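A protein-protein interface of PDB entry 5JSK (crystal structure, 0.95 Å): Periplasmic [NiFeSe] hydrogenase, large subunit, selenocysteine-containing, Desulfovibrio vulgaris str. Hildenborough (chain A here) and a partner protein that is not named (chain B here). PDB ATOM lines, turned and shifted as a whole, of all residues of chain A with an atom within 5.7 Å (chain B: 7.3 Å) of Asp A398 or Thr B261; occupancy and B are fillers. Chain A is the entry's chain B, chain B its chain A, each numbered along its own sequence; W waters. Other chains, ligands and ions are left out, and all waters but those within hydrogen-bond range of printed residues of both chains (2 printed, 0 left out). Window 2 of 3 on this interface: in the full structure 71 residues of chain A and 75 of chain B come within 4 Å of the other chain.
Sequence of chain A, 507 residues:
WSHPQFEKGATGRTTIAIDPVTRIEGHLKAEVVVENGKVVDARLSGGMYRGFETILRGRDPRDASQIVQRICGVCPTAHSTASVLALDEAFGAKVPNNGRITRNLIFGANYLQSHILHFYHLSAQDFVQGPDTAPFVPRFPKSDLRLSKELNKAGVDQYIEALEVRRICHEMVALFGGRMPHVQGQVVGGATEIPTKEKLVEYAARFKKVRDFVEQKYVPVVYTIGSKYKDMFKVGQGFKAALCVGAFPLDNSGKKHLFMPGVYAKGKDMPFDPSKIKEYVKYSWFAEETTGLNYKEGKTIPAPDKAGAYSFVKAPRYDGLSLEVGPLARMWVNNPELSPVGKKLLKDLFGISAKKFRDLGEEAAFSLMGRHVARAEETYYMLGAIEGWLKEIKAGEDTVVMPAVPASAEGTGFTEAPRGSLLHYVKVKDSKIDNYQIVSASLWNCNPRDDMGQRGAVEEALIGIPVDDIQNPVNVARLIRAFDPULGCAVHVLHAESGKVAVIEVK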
ATOM      1  N   PRO A  96      14.612 -16.045   1.663  1.00  0.00           N
ATOM      2  CA  PRO A  96      15.773 -15.699   0.839  1.00  0.00           C
ATOM      3  C   PRO A  96      16.062 -14.211   0.888  1.00  0.00           C
ATOM      4  O   PRO A  96      15.153 -13.388   0.995  1.00  0.00           O
ATOM      5  CB  PRO A  96      15.348 -16.135  -0.568  1.00  0.00           C
ATOM      6  CG  PRO A  96      14.294 -17.184  -0.357  1.00  0.00           C
ATOM      7  CD  PRO A  96      13.568 -16.729   0.880  1.00  0.00           C
ATOM      8  N   ASN A  97      17.339 -13.866   0.755  1.00  0.00           N
ATOM      9  CA  ASN A  97      17.743 -12.469   0.769  1.00  0.00           C
ATOM     10  C   ASN A  97      16.895 -11.624  -0.179  1.00  0.00           C
ATOM     11  O   ASN A  97      16.458 -10.528   0.175  1.00  0.00           O
ATOM     12  CB  ASN A  97      19.220 -12.376   0.392  1.00  0.00           C
ATOM     13  CG  ASN A  97      19.773 -10.987   0.570  1.00  0.00           C
ATOM     14  OD1 ASN A  97      19.834 -10.482   1.685  1.00  0.00           O
ATOM     15  ND2 ASN A  97      20.194 -10.368  -0.509  1.00  0.00           N
ATOM     16  N   ASN A  98      16.665 -12.110  -1.398  1.00  0.00           N
ATOM     17  CA  ASN A  98      15.924 -11.296  -2.360  1.00  0.00           C
ATOM     18  C   ASN A  98      14.472 -11.119  -1.941  1.00  0.00           C
ATOM     19  O   ASN A  98      13.844 -10.114  -2.295  1.00  0.00           O
ATOM     20  CB  ASN A  98      16.006 -11.891  -3.767  1.00  0.00           C
ATOM     21  CG  ASN A  98      16.043 -10.826  -4.837  1.00  0.00           C
ATOM     22  OD1 ASN A  98      16.798  -9.857  -4.727  1.00  0.00           O
ATOM     23  ND2 ASN A  98      15.261 -11.009  -5.890  1.00  0.00           N
ATOM     24  N   GLY A  99      13.929 -12.088  -1.205  1.00  0.00           N
ATOM     25  CA  GLY A  99      12.588 -11.948  -0.666  1.00  0.00           C
ATOM     26  C   GLY A  99      12.502 -10.937   0.459  1.00  0.00           C
ATOM     27  O   GLY A  99      11.502 -10.231   0.583  1.00  0.00           O
ATOM     28  N   ALA A 191       8.262 -13.705  -0.319  1.00  0.00           N
ATOM     29  CA  ALA A 191       7.413 -12.909  -1.197  1.00  0.00           C
ATOM     30  C   ALA A 191       7.060 -13.776  -2.394  1.00  0.00           C
ATOM     31  O   ALA A 191       7.910 -14.527  -2.886  1.00  0.00           O
ATOM     32  CB  ALA A 191       8.139 -11.634  -1.634  1.00  0.00           C
ATOM     33  N   THR A 192       5.808 -13.695  -2.842  1.00  0.00           N
ATOM     34  CA  THR A 192       5.269 -14.644  -3.809  1.00  0.00           C
ATOM     35  C   THR A 192       5.673 -14.368  -5.251  1.00  0.00           C
ATOM     36  O   THR A 192       5.438 -15.228  -6.110  1.00  0.00           O
ATOM     37  CB  THR A 192       3.741 -14.655  -3.736  1.00  0.00           C
ATOM     38  OG1 THR A 192       3.272 -13.343  -4.038  1.00  0.00           O
ATOM     39  CG2 THR A 192       3.245 -15.074  -2.371  1.00  0.00           C
ATOM     40  N   GLU A 193       6.251 -13.205  -5.542  1.00  0.00           N
ATOM     41  CA  GLU A 193       6.553 -12.814  -6.908  1.00  0.00           C
ATOM     42  C   GLU A 193       7.962 -12.245  -6.994  1.00  0.00           C
ATOM     43  O   GLU A 193       8.267 -11.202  -6.405  1.00  0.00           O
ATOM     44  CB  GLU A 193       5.520 -11.811  -7.431  1.00  0.00           C
ATOM     45  CG  GLU A 193       5.843 -11.324  -8.830  1.00  0.00           C
ATOM     46  CD  GLU A 193       4.809 -10.393  -9.429  1.00  0.00           C
ATOM     47  OE1 GLU A 193       3.726 -10.213  -8.855  1.00  0.00           O
ATOM     48  OE2 GLU A 193       5.106  -9.855 -10.518  1.00  0.00           O
ATOM     49  N   ILE A 194       8.800 -12.909  -7.769  1.00  0.00           N
ATOM     50  CA  ILE A 194      10.156 -12.425  -8.041  1.00  0.00           C
ATOM     51  C   ILE A 194      10.070 -11.132  -8.836  1.00  0.00           C
ATOM     52  O   ILE A 194       9.424 -11.119  -9.901  1.00  0.00           O
ATOM     53  CB  ILE A 194      10.921 -13.478  -8.849  1.00  0.00           C
ATOM     54  CG1 ILE A 194      11.136 -14.751  -8.027  1.00  0.00           C
ATOM     55  CG2 ILE A 194      12.232 -12.911  -9.361  1.00  0.00           C
ATOM     56  CD1 ILE A 194      11.658 -15.928  -8.835  1.00  0.00           C
ATOM     57  N   GLY A 396      14.985 -11.331 -10.973  1.00  0.00           N
ATOM     58  CA  GLY A 396      14.995 -12.731 -11.326  1.00  0.00           C
ATOM     59  C   GLY A 396      15.366 -13.704 -10.227  1.00  0.00           C
ATOM     60  O   GLY A 396      15.197 -14.913 -10.418  1.00  0.00           O
ATOM     61  N   GLU A 397      15.868 -13.239  -9.085  1.00  0.00           N
ATOM     62  CA  GLU A 397      16.322 -14.149  -8.042  1.00  0.00           C
ATOM     63  C   GLU A 397      15.181 -14.527  -7.104  1.00  0.00           C
ATOM     64  O   GLU A 397      14.357 -13.686  -6.744  1.00  0.00           O
ATOM     65  CB  GLU A 397      17.488 -13.531  -7.270  1.00  0.00           C
ATOM     66  CG  GLU A 397      18.763 -13.493  -8.081  1.00  0.00           C
ATOM     67  CD  GLU A 397      19.169 -14.868  -8.587  1.00  0.00           C
ATOM     68  OE1 GLU A 397      19.316 -15.020  -9.812  1.00  0.00           O
ATOM     69  OE2 GLU A 397      19.318 -15.802  -7.771  1.00  0.00           O
ATOM     70  N   ASP A 398      15.140 -15.807  -6.717  1.00  0.00           N
ATOM     71  CA  ASP A 398      13.981 -16.328  -5.995  1.00  0.00           C
ATOM     72  C   ASP A 398      13.779 -15.595  -4.668  1.00  0.00           C
ATOM     73  O   ASP A 398      14.718 -15.162  -3.993  1.00  0.00           O
ATOM     74  CB  ASP A 398      14.078 -17.838  -5.769  1.00  0.00           C
ATOM     75  CG  ASP A 398      12.696 -18.543  -5.640  1.00  0.00           C
ATOM     76  OD1 ASP A 398      11.631 -17.890  -5.458  1.00  0.00           O
ATOM     77  OD2 ASP A 398      12.697 -19.798  -5.706  1.00  0.00           O
ATOM     78  N   THR A 399      12.516 -15.449  -4.310  1.00  0.00           N
ATOM     79  CA  THR A 399      12.081 -14.666  -3.170  1.00  0.00           C
ATOM     80  C   THR A 399      11.308 -15.463  -2.130  1.00  0.00           C
ATOM     81  O   THR A 399      10.887 -14.871  -1.128  1.00  0.00           O
ATOM     82  CB  THR A 399      11.187 -13.513  -3.670  1.00  0.00           C
ATOM     83  OG1 THR A 399      10.150 -14.038  -4.510  1.00  0.00           O
ATOM     84  CG2 THR A 399      11.979 -12.497  -4.456  1.00  0.00           C
ATOM     85  N   VAL A 400      11.097 -16.771  -2.314  1.00  0.00           N
ATOM     86  CA  VAL A 400      10.267 -17.534  -1.388  1.00  0.00           C
ATOM     87  C   VAL A 400      10.823 -18.936  -1.185  1.00  0.00           C
ATOM     88  O   VAL A 400      11.412 -19.529  -2.095  1.00  0.00           O
ATOM     89  CB  VAL A 400       8.784 -17.578  -1.851  1.00  0.00           C
ATOM     90  CG1 VAL A 400       8.521 -18.718  -2.829  1.00  0.00           C
ATOM     91  CG2 VAL A 400       7.833 -17.633  -0.669  1.00  0.00           C
ATOM     92  N   SER B 257       1.983 -25.144 -10.382  1.00  0.00           N
ATOM     93  CA  SER B 257       3.149 -24.604  -9.693  1.00  0.00           C
ATOM     94  C   SER B 257       3.270 -25.191  -8.291  1.00  0.00           C
ATOM     95  O   SER B 257       2.280 -25.327  -7.566  1.00  0.00           O
ATOM     96  CB  SER B 257       3.043 -23.089  -9.618  1.00  0.00           C
ATOM     97  OG  SER B 257       3.099 -22.570 -10.931  1.00  0.00           O
ATOM     98  N   ALA B 258       4.505 -25.512  -7.899  1.00  0.00           N
ATOM     99  CA  ALA B 258       4.789 -26.037  -6.570  1.00  0.00           C
ATOM    100  C   ALA B 258       5.343 -24.973  -5.636  1.00  0.00           C
ATOM    101  O   ALA B 258       5.410 -25.200  -4.423  1.00  0.00           O
ATOM    102  CB  ALA B 258       5.783 -27.201  -6.652  1.00  0.00           C
ATOM    103  N   THR B 259       5.725 -23.824  -6.175  1.00  0.00           N
ATOM    104  CA  THR B 259       6.146 -22.677  -5.395  1.00  0.00           C
ATOM    105  C   THR B 259       5.446 -21.456  -5.962  1.00  0.00           C
ATOM    106  O   THR B 259       5.185 -21.374  -7.160  1.00  0.00           O
ATOM    107  CB  THR B 259       7.663 -22.460  -5.426  1.00  0.00           C
ATOM    108  OG1 THR B 259       7.946 -21.222  -4.778  1.00  0.00           O
ATOM    109  CG2 THR B 259       8.217 -22.426  -6.835  1.00  0.00           C
ATOM    110  N   PHE B 260       5.137 -20.507  -5.084  1.00  0.00           N
ATOM    111  CA  PHE B 260       4.449 -19.305  -5.533  1.00  0.00           C
ATOM    112  C   PHE B 260       5.185 -18.602  -6.660  1.00  0.00           C
ATOM    113  O   PHE B 260       4.550 -17.984  -7.520  1.00  0.00           O
ATOM    114  CB  PHE B 260       4.277 -18.307  -4.382  1.00  0.00           C
ATOM    115  CG  PHE B 260       3.319 -18.754  -3.310  1.00  0.00           C
ATOM    116  CD1 PHE B 260       1.955 -18.778  -3.536  1.00  0.00           C
ATOM    117  CD2 PHE B 260       3.786 -19.119  -2.055  1.00  0.00           C
ATOM    118  CE1 PHE B 260       1.082 -19.176  -2.533  1.00  0.00           C
ATOM    119  CE2 PHE B 260       2.915 -19.522  -1.065  1.00  0.00           C
ATOM    120  CZ  PHE B 260       1.570 -19.551  -1.302  1.00  0.00           C
ATOM    121  N   THR B 261       6.513 -18.644  -6.661  1.00  0.00           N
ATOM    122  CA  THR B 261       7.267 -17.844  -7.619  1.00  0.00           C
ATOM    123  C   THR B 261       7.355 -18.462  -9.009  1.00  0.00           C
ATOM    124  O   THR B 261       7.868 -17.803  -9.920  1.00  0.00           O
ATOM    125  CB  THR B 261       8.652 -17.521  -7.064  1.00  0.00           C
ATOM    126  OG1 THR B 261       9.281 -18.735  -6.661  1.00  0.00           O
ATOM    127  CG2 THR B 261       8.551 -16.566  -5.877  1.00  0.00           C
ATOM    128  N   ASP B 262       6.850 -19.685  -9.197  1.00  0.00           N
ATOM    129  CA  ASP B 262       6.718 -20.295 -10.526  1.00  0.00           C
ATOM    130  C   ASP B 262       5.458 -19.728 -11.167  1.00  0.00           C
ATOM    131  O   ASP B 262       4.339 -20.101 -10.802  1.00  0.00           O
ATOM    132  CB  ASP B 262       6.631 -21.814 -10.402  1.00  0.00           C
ATOM    133  CG  ASP B 262       6.377 -22.511 -11.724  1.00  0.00           C
ATOM    134  OD1 ASP B 262       6.158 -21.848 -12.758  1.00  0.00           O
ATOM    135  OD2 ASP B 262       6.407 -23.758 -11.733  1.00  0.00           O
ATOM    136  N   LYS B 263       5.630 -18.801 -12.105  1.00  0.00           N
ATOM    137  CA  LYS B 263       4.499 -18.134 -12.727  1.00  0.00           C
ATOM    138  C   LYS B 263       4.015 -18.826 -13.989  1.00  0.00           C
ATOM    139  O   LYS B 263       3.079 -18.329 -14.625  1.00  0.00           O
ATOM    140  CB  LYS B 263       4.834 -16.665 -13.006  1.00  0.00           C
ATOM    141  CG  LYS B 263       5.226 -15.869 -11.771  1.00  0.00           C
ATOM    142  CD  LYS B 263       4.264 -16.100 -10.610  1.00  0.00           C
ATOM    143  CE  LYS B 263       4.422 -15.086  -9.508  1.00  0.00           C
ATOM    144  NZ  LYS B 263       3.566 -15.461  -8.347  1.00  0.00           N
ATOM    145  N   VAL B 264       4.599 -19.972 -14.340  1.00  0.00           N
ATOM    146  CA  VAL B 264       4.169 -20.694 -15.532  1.00  0.00           C
ATOM    147  C   VAL B 264       2.955 -21.571 -15.246  1.00  0.00           C
ATOM    148  O   VAL B 264       2.018 -21.627 -16.049  1.00  0.00           O
ATOM    149  CB  VAL B 264       5.337 -21.503 -16.123  1.00  0.00           C
ATOM    150  CG1 VAL B 264       4.848 -22.367 -17.287  1.00  0.00           C
ATOM    151  CG2 VAL B 264       6.437 -20.561 -16.581  1.00  0.00           C
ATOM    152  N   ARG B 267      -2.142 -22.158 -10.372  1.00  0.00           N
ATOM    153  CA  ARG B 267      -2.032 -21.909  -8.943  1.00  0.00           C
ATOM    154  C   ARG B 267      -2.978 -22.760  -8.095  1.00  0.00           C
ATOM    155  O   ARG B 267      -3.052 -22.562  -6.880  1.00  0.00           O
ATOM    156  CB  ARG B 267      -2.271 -20.416  -8.666  1.00  0.00           C
ATOM    157  CG  ARG B 267      -1.160 -19.470  -9.104  1.00  0.00           C
ATOM    158  CD  ARG B 267      -0.970 -19.326 -10.610  1.00  0.00           C
ATOM    159  NE  ARG B 267      -0.299 -18.063 -10.888  1.00  0.00           N
ATOM    160  CZ  ARG B 267       0.501 -17.799 -11.910  1.00  0.00           C
ATOM    161  NH1 ARG B 267       0.802 -18.724 -12.813  1.00  0.00           N
ATOM    162  NH2 ARG B 267       1.020 -16.586 -12.026  1.00  0.00           N
ATOM    163  N   LEU B 270      -1.621 -24.446  -4.976  1.00  0.00           N
ATOM    164  CA  LEU B 270      -1.230 -23.434  -4.004  1.00  0.00           C
ATOM    165  C   LEU B 270      -2.429 -22.792  -3.315  1.00  0.00           C
ATOM    166  O   LEU B 270      -2.234 -21.946  -2.440  1.00  0.00           O
ATOM    167  CB  LEU B 270      -0.394 -22.365  -4.703  1.00  0.00           C
ATOM    168  CG  LEU B 270       0.961 -22.799  -5.253  1.00  0.00           C
ATOM    169  CD1 LEU B 270       1.504 -21.764  -6.220  1.00  0.00           C
ATOM    170  CD2 LEU B 270       1.960 -23.004  -4.112  1.00  0.00           C
ATOM    171  N   ASN B 296       0.028 -12.770  -9.054  1.00  0.00           N
ATOM    172  CA  ASN B 296       0.981 -12.516  -7.980  1.00  0.00           C
ATOM    173  C   ASN B 296       1.091 -13.672  -6.997  1.00  0.00           C
ATOM    174  O   ASN B 296       2.175 -13.939  -6.465  1.00  0.00           O
ATOM    175  CB  ASN B 296       0.516 -11.255  -7.238  1.00  0.00           C
ATOM    176  CG  ASN B 296       1.317 -10.936  -6.003  1.00  0.00           C
ATOM    177  OD1 ASN B 296       0.813 -11.010  -4.887  1.00  0.00           O
ATOM    178  ND2 ASN B 296       2.567 -10.541  -6.198  1.00  0.00           N
HETATM  179  O   HOH W   1      10.675 -21.092  -4.341  1.00  0.00           O
HETATM  180  O   HOH W   2       7.832 -15.043  -9.449  1.00  0.00           O
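The side-chain hydroxyl (OG1) of Thr B261 lies within hydrogen-bond range of the side-chain carboxylate (OD1) of Asp A398, 2.8 Å away.
The backbone carbonyl oxygen (O) of Thr A192 lies within hydrogen-bond range of the side-chain amino group (NZ) of Lys B263 (2.9 Å).
The backbone carbonyl oxygen (O) of Asn B296 sits at hydrogen-bond distance from the side-chain hydroxyl (OG1) of Thr A192 (2.7 Å).
ND2 of Asn B296 is in hydrogen-bond range of OE1 of Glu A193, at 2.9 Å.
The backbone carbonyl oxygen of Thr A192 lies close to the backbone carbonyl oxygen of Phe B260 (3.2 Å).
The side-chain hydroxyl (OG1) of Thr B261 lies within hydrogen-bond range of the side-chain hydroxyl (OG1) of Thr B259.
The side-chain amino group (NZ) of Lys B263 sits at hydrogen-bond distance from the backbone carbonyl oxygen (O) of Phe B260, 2.8 Å away.
NH1 of Arg B267 is in hydrogen-bond range of O of Lys B263, 2.9 Å away.
NZ of Lys B263 sits at hydrogen-bond distance from O of Asn B296.
O of Ala A191 sits at hydrogen-bond distance from OG1 of Thr A399, at 2.8 Å.
OD1 of Asp A398 sits at hydrogen-bond distance from N of Val A400.
O of Ala A191 touches CG2 of Thr B261 (3.7 Å).
Thr B261 touches Thr A192 (CG2 to O, 3.4 Å).
Ile A194 touches Thr B261 (CG1 to CG2, 3.8 Å).
Thr A399 touches Thr B261.
Val A400 touches Thr B259.
Val A400 touches Thr B261 (CG1 to CG2, 3.7 Å).
Printed residues of chain B within 4 Å of Glu A193: Asn B296.
Of the printed residues of chain B, Ile A194 touches Thr B261 (3.8 Å).
Asp A398 touches one residue of chain B.
Printed residues of chain A within 4 Å of Lys B263: Thr A192 (2.9 Å).
Arg B267 touches none of the printed residues of chain A.
Printed residues of chain A within 4 Å of Asn B296: Thr A192 and Glu A193.
The nearest residue of chain A that does not touch Thr B261 is Glu A193 (4.1 Å).
Printed residues of chain B that touch a printed residue of chain A: Thr B259, Phe B260, Thr B261, Lys B263 and Asn B296.
Hydrophobic or aromatic side chains of chain B that line the printed part of chain A: Phe B260.
Of the 13 printed residues of chain A, 7 touch a printed residue of chain B.
Hydrophobic or aromatic side chains of chain A within 4 Å of the printed part of chain B: Ile A194 and Val A400.
Along chain A the printed residues that touch a printed residue of chain B span positions 191 to 400.
Among the printed residues, no Asp or Glu carboxylate lies within 4 Å of a Lys or Arg side-chain nitrogen of the other chain.
Water W1 lies within hydrogen-bond range of OD2 of Asp A398 (2.8 Å), OG1 of Thr B259 (2.8 Å) and O of Val A400 (2.8 Å).
Water W2 bridges O of Thr B261 (2.8 Å) and N of Ile A194 (2.9 Å).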
